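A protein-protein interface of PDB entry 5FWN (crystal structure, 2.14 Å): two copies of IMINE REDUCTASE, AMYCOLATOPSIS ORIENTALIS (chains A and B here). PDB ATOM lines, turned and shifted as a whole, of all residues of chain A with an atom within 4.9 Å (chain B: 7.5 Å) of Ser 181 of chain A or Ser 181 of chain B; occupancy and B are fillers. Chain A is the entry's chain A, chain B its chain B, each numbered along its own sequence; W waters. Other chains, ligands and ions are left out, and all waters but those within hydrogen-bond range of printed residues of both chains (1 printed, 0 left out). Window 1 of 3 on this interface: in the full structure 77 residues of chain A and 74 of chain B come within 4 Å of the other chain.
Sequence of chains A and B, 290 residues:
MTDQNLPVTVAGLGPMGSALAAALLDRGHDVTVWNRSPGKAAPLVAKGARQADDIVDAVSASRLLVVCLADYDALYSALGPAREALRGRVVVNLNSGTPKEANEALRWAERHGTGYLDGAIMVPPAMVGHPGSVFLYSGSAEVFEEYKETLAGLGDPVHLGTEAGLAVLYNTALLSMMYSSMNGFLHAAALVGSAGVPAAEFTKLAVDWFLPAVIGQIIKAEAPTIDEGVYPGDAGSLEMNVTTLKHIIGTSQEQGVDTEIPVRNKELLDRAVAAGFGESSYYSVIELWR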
ATOM      1  N   MET A 177       1.459  -7.179   3.092  1.00  0.00           N
ATOM      2  CA  MET A 177       1.238  -7.435   1.675  1.00  0.00           C
ATOM      3  C   MET A 177       2.412  -6.939   0.791  1.00  0.00           C
ATOM      4  O   MET A 177       2.803  -7.591  -0.177  1.00  0.00           O
ATOM      5  CB  MET A 177      -0.071  -6.775   1.252  1.00  0.00           C
ATOM      6  CG  MET A 177      -0.423  -6.885  -0.248  1.00  0.00           C
ATOM      7  SD  MET A 177      -1.828  -5.833  -0.671  1.00  0.00           S
ATOM      8  CE  MET A 177      -1.906  -6.153  -2.427  1.00  0.00           C
ATOM      9  N   MET A 178       2.909  -5.744   1.090  1.00  0.00           N
ATOM     10  CA  MET A 178       4.039  -5.173   0.362  1.00  0.00           C
ATOM     11  C   MET A 178       5.262  -6.086   0.383  1.00  0.00           C
ATOM     12  O   MET A 178       5.853  -6.337  -0.682  1.00  0.00           O
ATOM     13  CB  MET A 178       4.426  -3.788   0.912  1.00  0.00           C
ATOM     14  CG  MET A 178       5.585  -3.109   0.167  1.00  0.00           C
ATOM     15  SD  MET A 178       6.056  -1.563   0.966  1.00  0.00           S
ATOM     16  CE  MET A 178       7.028  -2.336   2.287  1.00  0.00           C
ATOM     17  N   TYR A 179       5.660  -6.560   1.579  1.00  0.00           N
ATOM     18  CA  TYR A 179       6.823  -7.430   1.643  1.00  0.00           C
ATOM     19  C   TYR A 179       6.659  -8.674   0.800  1.00  0.00           C
ATOM     20  O   TYR A 179       7.542  -8.995  -0.004  1.00  0.00           O
ATOM     21  CB  TYR A 179       7.241  -7.770   3.085  1.00  0.00           C
ATOM     22  CG  TYR A 179       7.734  -6.557   3.806  1.00  0.00           C
ATOM     23  CD1 TYR A 179       8.941  -5.938   3.444  1.00  0.00           C
ATOM     24  CD2 TYR A 179       7.043  -6.018   4.853  1.00  0.00           C
ATOM     25  CE1 TYR A 179       9.402  -4.805   4.119  1.00  0.00           C
ATOM     26  CE2 TYR A 179       7.490  -4.860   5.506  1.00  0.00           C
ATOM     27  CZ  TYR A 179       8.662  -4.271   5.158  1.00  0.00           C
ATOM     28  OH  TYR A 179       9.105  -3.151   5.839  1.00  0.00           O
ATOM     29  N   SER A 180       5.510  -9.328   0.901  1.00  0.00           N
ATOM     30  CA  SER A 180       5.269 -10.517   0.084  1.00  0.00           C
ATOM     31  C   SER A 180       5.309 -10.216  -1.417  1.00  0.00           C
ATOM     32  O   SER A 180       5.904 -10.974  -2.173  1.00  0.00           O
ATOM     33  CB  SER A 180       3.942 -11.139   0.431  1.00  0.00           C
ATOM     34  OG  SER A 180       3.986 -11.833   1.686  1.00  0.00           O
ATOM     35  N   SER A 181       4.695  -9.100  -1.831  1.00  0.00           N
ATOM     36  CA  SER A 181       4.667  -8.715  -3.239  1.00  0.00           C
ATOM     37  C   SER A 181       6.053  -8.433  -3.776  1.00  0.00           C
ATOM     38  O   SER A 181       6.375  -8.861  -4.869  1.00  0.00           O
ATOM     39  CB  SER A 181       3.773  -7.494  -3.544  1.00  0.00           C
ATOM     40  OG  SER A 181       2.504  -7.651  -2.946  1.00  0.00           O
ATOM     41  N   MET A 182       6.832  -7.664  -3.027  1.00  0.00           N
ATOM     42  CA  MET A 182       8.169  -7.341  -3.448  1.00  0.00           C
ATOM     43  C   MET A 182       8.998  -8.611  -3.587  1.00  0.00           C
ATOM     44  O   MET A 182       9.821  -8.711  -4.459  1.00  0.00           O
ATOM     45  CB  MET A 182       8.851  -6.394  -2.461  1.00  0.00           C
ATOM     46  CG  MET A 182       8.262  -5.000  -2.473  1.00  0.00           C
ATOM     47  SD  MET A 182       9.291  -3.870  -1.549  1.00  0.00           S
ATOM     48  CE  MET A 182       9.165  -4.608   0.052  1.00  0.00           C
ATOM     49  N   ASN A 183       8.854  -9.543  -2.652  1.00  0.00           N
ATOM     50  CA  ASN A 183       9.635 -10.777  -2.717  1.00  0.00           C
ATOM     51  C   ASN A 183       9.288 -11.632  -3.901  1.00  0.00           C
ATOM     52  O   ASN A 183      10.168 -12.242  -4.511  1.00  0.00           O
ATOM     53  CB  ASN A 183       9.540 -11.597  -1.400  1.00  0.00           C
ATOM     54  CG  ASN A 183      10.112 -10.849  -0.171  1.00  0.00           C
ATOM     55  OD1 ASN A 183       9.772 -11.173   1.008  1.00  0.00           O
ATOM     56  ND2 ASN A 183      10.921  -9.862  -0.397  1.00  0.00           N
ATOM     57  N   GLY A 184       7.995 -11.714  -4.212  1.00  0.00           N
ATOM     58  CA  GLY A 184       7.562 -12.399  -5.398  1.00  0.00           C
ATOM     59  C   GLY A 184       8.056 -11.725  -6.662  1.00  0.00           C
ATOM     60  O   GLY A 184       8.522 -12.386  -7.579  1.00  0.00           O
ATOM     61  N   PHE A 185       8.028 -10.391  -6.680  1.00  0.00           N
ATOM     62  CA  PHE A 185       8.645  -9.649  -7.783  1.00  0.00           C
ATOM     63  C   PHE A 185      10.141 -10.010  -7.958  1.00  0.00           C
ATOM     64  O   PHE A 185      10.603 -10.135  -9.064  1.00  0.00           O
ATOM     65  CB  PHE A 185       8.554  -8.125  -7.592  1.00  0.00           C
ATOM     66  CG  PHE A 185       9.356  -7.384  -8.610  1.00  0.00           C
ATOM     67  CD1 PHE A 185       8.882  -7.286  -9.924  1.00  0.00           C
ATOM     68  CD2 PHE A 185      10.620  -6.939  -8.329  1.00  0.00           C
ATOM     69  CE1 PHE A 185       9.659  -6.712 -10.901  1.00  0.00           C
ATOM     70  CE2 PHE A 185      11.382  -6.331  -9.325  1.00  0.00           C
ATOM     71  CZ  PHE A 185      10.906  -6.247 -10.603  1.00  0.00           C
ATOM     72  N   ILE A 215      -2.928  -8.595 -10.985  1.00  0.00           N
ATOM     73  CA  ILE A 215      -2.890  -8.897  -9.548  1.00  0.00           C
ATOM     74  C   ILE A 215      -4.070  -8.180  -8.803  1.00  0.00           C
ATOM     75  O   ILE A 215      -4.826  -8.812  -8.076  1.00  0.00           O
ATOM     76  CB  ILE A 215      -1.522  -8.568  -8.951  1.00  0.00           C
ATOM     77  CG1 ILE A 215      -0.438  -9.458  -9.585  1.00  0.00           C
ATOM     78  CG2 ILE A 215      -1.526  -8.713  -7.417  1.00  0.00           C
ATOM     79  CD1 ILE A 215       1.013  -9.134  -9.114  1.00  0.00           C
ATOM     80  N   ILE A 219      -7.290 -10.216  -7.103  1.00  0.00           N
ATOM     81  CA  ILE A 219      -7.579 -10.011  -5.681  1.00  0.00           C
ATOM     82  C   ILE A 219      -9.043  -9.611  -5.492  1.00  0.00           C
ATOM     83  O   ILE A 219      -9.739 -10.272  -4.743  1.00  0.00           O
ATOM     84  CB  ILE A 219      -6.644  -8.954  -5.019  1.00  0.00           C
ATOM     85  CG1 ILE A 219      -5.274  -9.595  -4.814  1.00  0.00           C
ATOM     86  CG2 ILE A 219      -7.213  -8.447  -3.689  1.00  0.00           C
ATOM     87  CD1 ILE A 219      -4.163  -8.630  -4.483  1.00  0.00           C
ATOM     88  N   LEU B 174       5.711 -13.676 -13.919  1.00  0.00           N
ATOM     89  CA  LEU B 174       4.651 -12.812 -13.486  1.00  0.00           C
ATOM     90  C   LEU B 174       3.727 -13.565 -12.553  1.00  0.00           C
ATOM     91  O   LEU B 174       3.338 -13.042 -11.523  1.00  0.00           O
ATOM     92  CB  LEU B 174       3.882 -12.237 -14.670  1.00  0.00           C
ATOM     93  CG  LEU B 174       4.718 -11.239 -15.487  1.00  0.00           C
ATOM     94  CD1 LEU B 174       3.980 -10.961 -16.787  1.00  0.00           C
ATOM     95  CD2 LEU B 174       5.019  -9.941 -14.761  1.00  0.00           C
ATOM     96  N   LEU B 175       3.379 -14.806 -12.876  1.00  0.00           N
ATOM     97  CA  LEU B 175       2.473 -15.535 -12.021  1.00  0.00           C
ATOM     98  C   LEU B 175       3.124 -15.803 -10.650  1.00  0.00           C
ATOM     99  O   LEU B 175       2.440 -15.816  -9.628  1.00  0.00           O
ATOM    100  CB  LEU B 175       1.969 -16.806 -12.698  1.00  0.00           C
ATOM    101  CG  LEU B 175       1.091 -16.656 -13.940  1.00  0.00           C
ATOM    102  CD1 LEU B 175       0.826 -18.030 -14.616  1.00  0.00           C
ATOM    103  CD2 LEU B 175      -0.242 -16.020 -13.581  1.00  0.00           C
ATOM    104  N   SER B 176       4.434 -16.054 -10.640  1.00  0.00           N
ATOM    105  CA  SER B 176       5.131 -16.292  -9.365  1.00  0.00           C
ATOM    106  C   SER B 176       4.952 -15.075  -8.465  1.00  0.00           C
ATOM    107  O   SER B 176       4.625 -15.219  -7.298  1.00  0.00           O
ATOM    108  CB  SER B 176       6.599 -16.604  -9.589  1.00  0.00           C
ATOM    109  OG  SER B 176       7.197 -17.087  -8.425  1.00  0.00           O
ATOM    110  N   MET B 177       5.117 -13.881  -9.021  1.00  0.00           N
ATOM    111  CA  MET B 177       4.870 -12.650  -8.300  1.00  0.00           C
ATOM    112  C   MET B 177       3.420 -12.536  -7.852  1.00  0.00           C
ATOM    113  O   MET B 177       3.125 -12.105  -6.717  1.00  0.00           O
ATOM    114  CB  MET B 177       5.287 -11.443  -9.136  1.00  0.00           C
ATOM    115  CG  MET B 177       4.971 -10.068  -8.544  1.00  0.00           C
ATOM    116  SD  MET B 177       5.196  -8.738  -9.799  1.00  0.00           S
ATOM    117  CE  MET B 177       4.733  -7.322  -8.755  1.00  0.00           C
ATOM    118  N   MET B 178       2.498 -12.923  -8.728  1.00  0.00           N
ATOM    119  CA  MET B 178       1.042 -12.885  -8.395  1.00  0.00           C
ATOM    120  C   MET B 178       0.712 -13.744  -7.169  1.00  0.00           C
ATOM    121  O   MET B 178       0.032 -13.277  -6.267  1.00  0.00           O
ATOM    122  CB  MET B 178       0.200 -13.349  -9.573  1.00  0.00           C
ATOM    123  CG  MET B 178      -1.290 -13.343  -9.308  1.00  0.00           C
ATOM    124  SD  MET B 178      -2.197 -14.045 -10.665  1.00  0.00           S
ATOM    125  CE  MET B 178      -1.930 -15.776 -10.249  1.00  0.00           C
ATOM    126  N   TYR B 179       1.180 -14.996  -7.152  1.00  0.00           N
ATOM    127  CA  TYR B 179       0.903 -15.814  -6.006  1.00  0.00           C
ATOM    128  C   TYR B 179       1.403 -15.211  -4.725  1.00  0.00           C
ATOM    129  O   TYR B 179       0.659 -15.180  -3.742  1.00  0.00           O
ATOM    130  CB  TYR B 179       1.377 -17.270  -6.146  1.00  0.00           C
ATOM    131  CG  TYR B 179       0.594 -18.001  -7.229  1.00  0.00           C
ATOM    132  CD1 TYR B 179      -0.765 -18.299  -7.071  1.00  0.00           C
ATOM    133  CD2 TYR B 179       1.200 -18.370  -8.417  1.00  0.00           C
ATOM    134  CE1 TYR B 179      -1.481 -18.969  -8.069  1.00  0.00           C
ATOM    135  CE2 TYR B 179       0.491 -19.037  -9.407  1.00  0.00           C
ATOM    136  CZ  TYR B 179      -0.846 -19.324  -9.244  1.00  0.00           C
ATOM    137  OH  TYR B 179      -1.510 -19.934 -10.255  1.00  0.00           O
ATOM    138  N   SER B 180       2.635 -14.717  -4.717  1.00  0.00           N
ATOM    139  CA  SER B 180       3.173 -14.111  -3.486  1.00  0.00           C
ATOM    140  C   SER B 180       2.322 -12.885  -3.068  1.00  0.00           C
ATOM    141  O   SER B 180       2.023 -12.723  -1.889  1.00  0.00           O
ATOM    142  CB  SER B 180       4.615 -13.659  -3.693  1.00  0.00           C
ATOM    143  OG  SER B 180       5.502 -14.758  -3.671  1.00  0.00           O
ATOM    144  N   SER B 181       1.951 -12.057  -4.021  1.00  0.00           N
ATOM    145  CA  SER B 181       1.203 -10.831  -3.743  1.00  0.00           C
ATOM    146  C   SER B 181      -0.136 -11.151  -3.193  1.00  0.00           C
ATOM    147  O   SER B 181      -0.587 -10.491  -2.258  1.00  0.00           O
ATOM    148  CB  SER B 181       0.998  -9.919  -4.982  1.00  0.00           C
ATOM    149  OG  SER B 181       2.242  -9.687  -5.595  1.00  0.00           O
ATOM    150  N   MET B 182      -0.805 -12.148  -3.786  1.00  0.00           N
ATOM    151  CA  MET B 182      -2.130 -12.530  -3.341  1.00  0.00           C
ATOM    152  C   MET B 182      -2.044 -13.071  -1.903  1.00  0.00           C
ATOM    153  O   MET B 182      -2.918 -12.806  -1.101  1.00  0.00           O
ATOM    154  CB  MET B 182      -2.752 -13.611  -4.210  1.00  0.00           C
ATOM    155  CG  MET B 182      -3.157 -13.159  -5.602  1.00  0.00           C
ATOM    156  SD  MET B 182      -3.858 -14.608  -6.480  1.00  0.00           S
ATOM    157  CE  MET B 182      -5.481 -14.333  -5.763  1.00  0.00           C
ATOM    158  N   ASN B 183      -1.041 -13.906  -1.632  1.00  0.00           N
ATOM    159  CA  ASN B 183      -0.899 -14.472  -0.280  1.00  0.00           C
ATOM    160  C   ASN B 183      -0.630 -13.402   0.756  1.00  0.00           C
ATOM    161  O   ASN B 183      -1.155 -13.447   1.865  1.00  0.00           O
ATOM    162  CB  ASN B 183       0.157 -15.582  -0.230  1.00  0.00           C
ATOM    163  CG  ASN B 183      -0.133 -16.754  -1.131  1.00  0.00           C
ATOM    164  OD1 ASN B 183       0.791 -17.545  -1.485  1.00  0.00           O
ATOM    165  ND2 ASN B 183      -1.371 -16.945  -1.485  1.00  0.00           N
ATOM    166  N   GLY B 184       0.217 -12.446   0.425  1.00  0.00           N
ATOM    167  CA  GLY B 184       0.421 -11.276   1.288  1.00  0.00           C
ATOM    168  C   GLY B 184      -0.879 -10.513   1.521  1.00  0.00           C
ATOM    169  O   GLY B 184      -1.161 -10.087   2.639  1.00  0.00           O
ATOM    170  N   PHE B 185      -1.635 -10.296   0.457  1.00  0.00           N
ATOM    171  CA  PHE B 185      -2.940  -9.636   0.605  1.00  0.00           C
ATOM    172  C   PHE B 185      -3.865 -10.406   1.553  1.00  0.00           C
ATOM    173  O   PHE B 185      -4.533  -9.798   2.372  1.00  0.00           O
ATOM    174  CB  PHE B 185      -3.662  -9.489  -0.699  1.00  0.00           C
ATOM    175  CG  PHE B 185      -5.064  -9.000  -0.488  1.00  0.00           C
ATOM    176  CD1 PHE B 185      -5.303  -7.653  -0.189  1.00  0.00           C
ATOM    177  CD2 PHE B 185      -6.095  -9.870  -0.476  1.00  0.00           C
ATOM    178  CE1 PHE B 185      -6.568  -7.198   0.085  1.00  0.00           C
ATOM    179  CE2 PHE B 185      -7.390  -9.419  -0.212  1.00  0.00           C
ATOM    180  CZ  PHE B 185      -7.616  -8.085   0.072  1.00  0.00           C
ATOM    181  N   LEU B 186      -3.876 -11.725   1.447  1.00  0.00           N
ATOM    182  CA  LEU B 186      -4.703 -12.519   2.345  1.00  0.00           C
ATOM    183  C   LEU B 186      -4.252 -12.446   3.799  1.00  0.00           C
ATOM    184  O   LEU B 186      -5.104 -12.395   4.668  1.00  0.00           O
ATOM    185  CB  LEU B 186      -4.817 -13.976   1.882  1.00  0.00           C
ATOM    186  CG  LEU B 186      -5.494 -14.185   0.507  1.00  0.00           C
ATOM    187  CD1 LEU B 186      -5.390 -15.650   0.092  1.00  0.00           C
ATOM    188  CD2 LEU B 186      -6.947 -13.722   0.457  1.00  0.00           C
ATOM    189  N   HIS B 187      -2.934 -12.378   4.059  1.00  0.00           N
ATOM    190  CA  HIS B 187      -2.460 -12.083   5.420  1.00  0.00           C
ATOM    191  C   HIS B 187      -2.970 -10.717   5.870  1.00  0.00           C
ATOM    192  O   HIS B 187      -3.607 -10.607   6.899  1.00  0.00           O
ATOM    193  CB  HIS B 187      -0.943 -12.185   5.565  1.00  0.00           C
ATOM    194  CG  HIS B 187      -0.492 -12.038   6.969  1.00  0.00           C
ATOM    195  ND1 HIS B 187       0.143 -10.919   7.410  1.00  0.00           N
ATOM    196  CD2 HIS B 187      -0.694 -12.802   8.060  1.00  0.00           C
ATOM    197  CE1 HIS B 187       0.349 -11.006   8.710  1.00  0.00           C
ATOM    198  NE2 HIS B 187      -0.103 -12.156   9.115  1.00  0.00           N
ATOM    199  N   PHE B 210      -3.008   1.411  -2.461  1.00  0.00           N
ATOM    200  CA  PHE B 210      -1.711   1.036  -1.914  1.00  0.00           C
ATOM    201  C   PHE B 210      -0.861   0.300  -2.948  1.00  0.00           C
ATOM    202  O   PHE B 210       0.351   0.533  -3.072  1.00  0.00           O
ATOM    203  CB  PHE B 210      -1.888   0.171  -0.674  1.00  0.00           C
ATOM    204  CG  PHE B 210      -0.608  -0.098   0.069  1.00  0.00           C
ATOM    205  CD1 PHE B 210      -0.018   0.877   0.823  1.00  0.00           C
ATOM    206  CD2 PHE B 210      -0.003  -1.354  -0.014  1.00  0.00           C
ATOM    207  CE1 PHE B 210       1.186   0.632   1.505  1.00  0.00           C
ATOM    208  CE2 PHE B 210       1.194  -1.607   0.642  1.00  0.00           C
ATOM    209  CZ  PHE B 210       1.804  -0.612   1.378  1.00  0.00           C
ATOM    210  N   LEU B 211      -1.488  -0.635  -3.658  1.00  0.00           N
ATOM    211  CA  LEU B 211      -0.770  -1.472  -4.629  1.00  0.00           C
ATOM    212  C   LEU B 211      -0.045  -0.623  -5.727  1.00  0.00           C
ATOM    213  O   LEU B 211       1.135  -0.775  -5.932  1.00  0.00           O
ATOM    214  CB  LEU B 211      -1.739  -2.517  -5.208  1.00  0.00           C
ATOM    215  CG  LEU B 211      -1.347  -3.506  -6.308  1.00  0.00           C
ATOM    216  CD1 LEU B 211      -2.366  -4.634  -6.441  1.00  0.00           C
ATOM    217  CD2 LEU B 211      -1.454  -2.733  -7.624  1.00  0.00           C
ATOM    218  N   ILE B 215       3.327  -0.001  -3.496  1.00  0.00           N
ATOM    219  CA  ILE B 215       4.065  -1.208  -3.856  1.00  0.00           C
ATOM    220  C   ILE B 215       4.766  -1.062  -5.236  1.00  0.00           C
ATOM    221  O   ILE B 215       5.969  -1.304  -5.368  1.00  0.00           O
ATOM    222  CB  ILE B 215       3.172  -2.468  -3.794  1.00  0.00           C
ATOM    223  CG1 ILE B 215       2.661  -2.701  -2.344  1.00  0.00           C
ATOM    224  CG2 ILE B 215       3.894  -3.714  -4.334  1.00  0.00           C
ATOM    225  CD1 ILE B 215       1.675  -3.887  -2.211  1.00  0.00           C
ATOM    226  N   GLY B 216       4.023  -0.640  -6.246  1.00  0.00           N
ATOM    227  CA  GLY B 216       4.587  -0.439  -7.584  1.00  0.00           C
ATOM    228  C   GLY B 216       5.747   0.537  -7.602  1.00  0.00           C
ATOM    229  O   GLY B 216       6.841   0.281  -8.187  1.00  0.00           O
ATOM    230  N   ILE B 219       8.881  -0.862  -5.758  1.00  0.00           N
ATOM    231  CA  ILE B 219       9.550  -1.820  -6.649  1.00  0.00           C
ATOM    232  C   ILE B 219      10.445  -1.091  -7.676  1.00  0.00           C
ATOM    233  O   ILE B 219      11.642  -1.373  -7.769  1.00  0.00           O
ATOM    234  CB  ILE B 219       8.562  -2.775  -7.338  1.00  0.00           C
ATOM    235  CG1 ILE B 219       8.066  -3.808  -6.319  1.00  0.00           C
ATOM    236  CG2 ILE B 219       9.210  -3.469  -8.532  1.00  0.00           C
ATOM    237  CD1 ILE B 219       6.859  -4.576  -6.763  1.00  0.00           C
ATOM    238  N   ASN B 265       8.930 -13.689   5.561  1.00  0.00           N
ATOM    239  CA  ASN B 265       9.468 -12.460   4.911  1.00  0.00           C
ATOM    240  C   ASN B 265      10.641 -11.872   5.761  1.00  0.00           C
ATOM    241  O   ASN B 265      11.696 -11.555   5.224  1.00  0.00           O
ATOM    242  CB  ASN B 265       8.364 -11.443   4.702  1.00  0.00           C
ATOM    243  CG  ASN B 265       7.382 -11.855   3.649  1.00  0.00           C
ATOM    244  OD1 ASN B 265       6.194 -11.486   3.705  1.00  0.00           O
ATOM    245  ND2 ASN B 265       7.826 -12.624   2.728  1.00  0.00           N
ATOM    246  N   TYR B 282      17.125  -3.253  -0.173  1.00  0.00           N
ATOM    247  CA  TYR B 282      16.086  -4.283  -0.227  1.00  0.00           C
ATOM    248  C   TYR B 282      16.288  -5.205  -1.472  1.00  0.00           C
ATOM    249  O   TYR B 282      16.235  -6.429  -1.377  1.00  0.00           O
ATOM    250  CB  TYR B 282      14.656  -3.683  -0.170  1.00  0.00           C
ATOM    251  CG  TYR B 282      13.650  -4.745   0.169  1.00  0.00           C
ATOM    252  CD1 TYR B 282      13.282  -5.714  -0.752  1.00  0.00           C
ATOM    253  CD2 TYR B 282      13.113  -4.828   1.450  1.00  0.00           C
ATOM    254  CE1 TYR B 282      12.382  -6.718  -0.426  1.00  0.00           C
ATOM    255  CE2 TYR B 282      12.244  -5.844   1.808  1.00  0.00           C
ATOM    256  CZ  TYR B 282      11.866  -6.779   0.860  1.00  0.00           C
ATOM    257  OH  TYR B 282      11.012  -7.797   1.242  1.00  0.00           O
HETATM  258  O   HOH W   1      10.545  -9.566   3.269  1.00  0.00           O
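The backbone carbonyl oxygen (O) of Met 177 of chain A sits at hydrogen-bond distance from the side-chain hydroxyl (OG) of Ser 181 of chain A, at 2.8 Å. The backbone carbonyl oxygen (O) of Tyr 179 of chain A lies close to the side-chain amide oxygen (OD1) of Asn 183 of chain A (3.3 Å). The side-chain hydroxyl (OG) of Ser 181 of chain B is in hydrogen-bond range of the backbone carbonyl oxygen (O) of Met 177 of chain B (2.8 Å). O of Phe 210 of chain B lies within hydrogen-bond range of N of Ile 215 of chain B (3.1 Å).
Among the printed residues, merely in contact across the chains: Ser 180 of chain A with Ser 180 of chain B (3.3 Å), Tyr 179 of chain A with Tyr 282 of chain B (3.5 Å), Met 182 of chain A with Tyr 282 of chain B (3.6 Å), Gly 184 of chain A with Ser 180 of chain B (3.6 Å), Phe 185 of chain A with Met 177 of chain B (3.6 Å), Ile 219 of chain A with Phe 185 of chain B (3.6 Å), Ser 180 of chain A with Gly 184 of chain B (3.6 Å), Phe 185 of chain A with Ile 219 of chain B (3.7 Å), Met 177 of chain A with Phe 185 of chain B (3.7 Å), Gly 184 of chain A with Met 177 of chain B (3.7 Å), Met 177 of chain A with Gly 184 of chain B (3.7 Å), Ile 215 of chain A with Ser 181 of chain B (3.7 Å), Met 178 of chain A with Ile 215 of chain B (3.7 Å), Ile 215 of chain A with Met 178 of chain B (3.8 Å), Ser 181 of chain A with Ile 215 of chain B (3.9 Å), Met 178 of chain A with Phe 210 of chain B (3.9 Å) and Tyr 179 of chain A with Asn 265 of chain B (3.9 Å).
Water W1 lies within hydrogen-bond range of the side-chain hydroxyl (OH) of Tyr 282 of chain B, the side-chain amide oxygen (OD1) of Asn 183 of chain A and the backbone carbonyl oxygen (O) of Asn 265 of chain B.
Printed residues of chain B that touch a printed residue of chain A: Met 177, Met 178, Ser 180, Ser 181, Gly 184, Phe 185, Phe 210, Ile 215, Ile 219, Asn 265 and Tyr 282. Hydrophobic or aromatic side chains of chain B that line the printed part of chain A: Met 177, Met 178, Phe 185, Phe 210, Ile 215, Ile 219 and Tyr 282. Among the printed residues, no Asp or Glu carboxylate lies within 4 Å of a Lys or Arg side-chain nitrogen of the other chain.
Of the printed residues of chain B, Met 177 of chain A touches Gly 184 (3.7 Å) and Phe 185 (3.7 Å). Of the printed residues of chain B, Ser 180 of chain A touches Ser 180, Gly 184 and Asn 265. Of the printed residues of chain B, Ser 181 of chain A touches Ser 181 and Ile 215. Printed residues of chain B within 4 Å of Gly 184 of chain A: Met 177 and Ser 180. Ser 181 of chain B touches just these residues of chain A: Ser 181 and Ile 215. Of the printed residues of chain A, Gly 184 of chain B touches Met 177 and Ser 180. The nearest residue of chain B that does not touch Ser 181 of chain A is Met 177 of chain B (4.1 Å).
The side-chain amide oxygen of Asn 265 of chain B sits at hydrogen-bond distance from the side-chain hydroxyl of Ser 180 of chain A, at 3.0 Å. OG of Ser 181 of chain B sits at hydrogen-bond distance from OG of Ser 181 of chain A (3.4 Å). OD1 of Asn 183 of chain A is in hydrogen-bond range of ND2 of Asn 265 of chain B, at 3.0 Å. The side-chain amide nitrogen of Asn 183 of chain A sits at hydrogen-bond distance from the side-chain hydroxyl of Tyr 282 of chain B (2.6 Å).
Met 177 of chain A touches Gly 184 of chain B, and with the chains exchanged Gly 184 of chain A touches Met 177 of chain B. Ser 180 of chain B touches its own counterpart, Ser 180 of chain A. Ser 180 of chain A touches Gly 184 of chain B, and with the chains exchanged Gly 184 of chain A touches Ser 180 of chain B. Ser 181 of chain A touches its own counterpart, Ser 181 of chain B. Of the 21 pairs that touch across the chains among the printed residues, 14 have their exchanged pair printed and touching as well.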
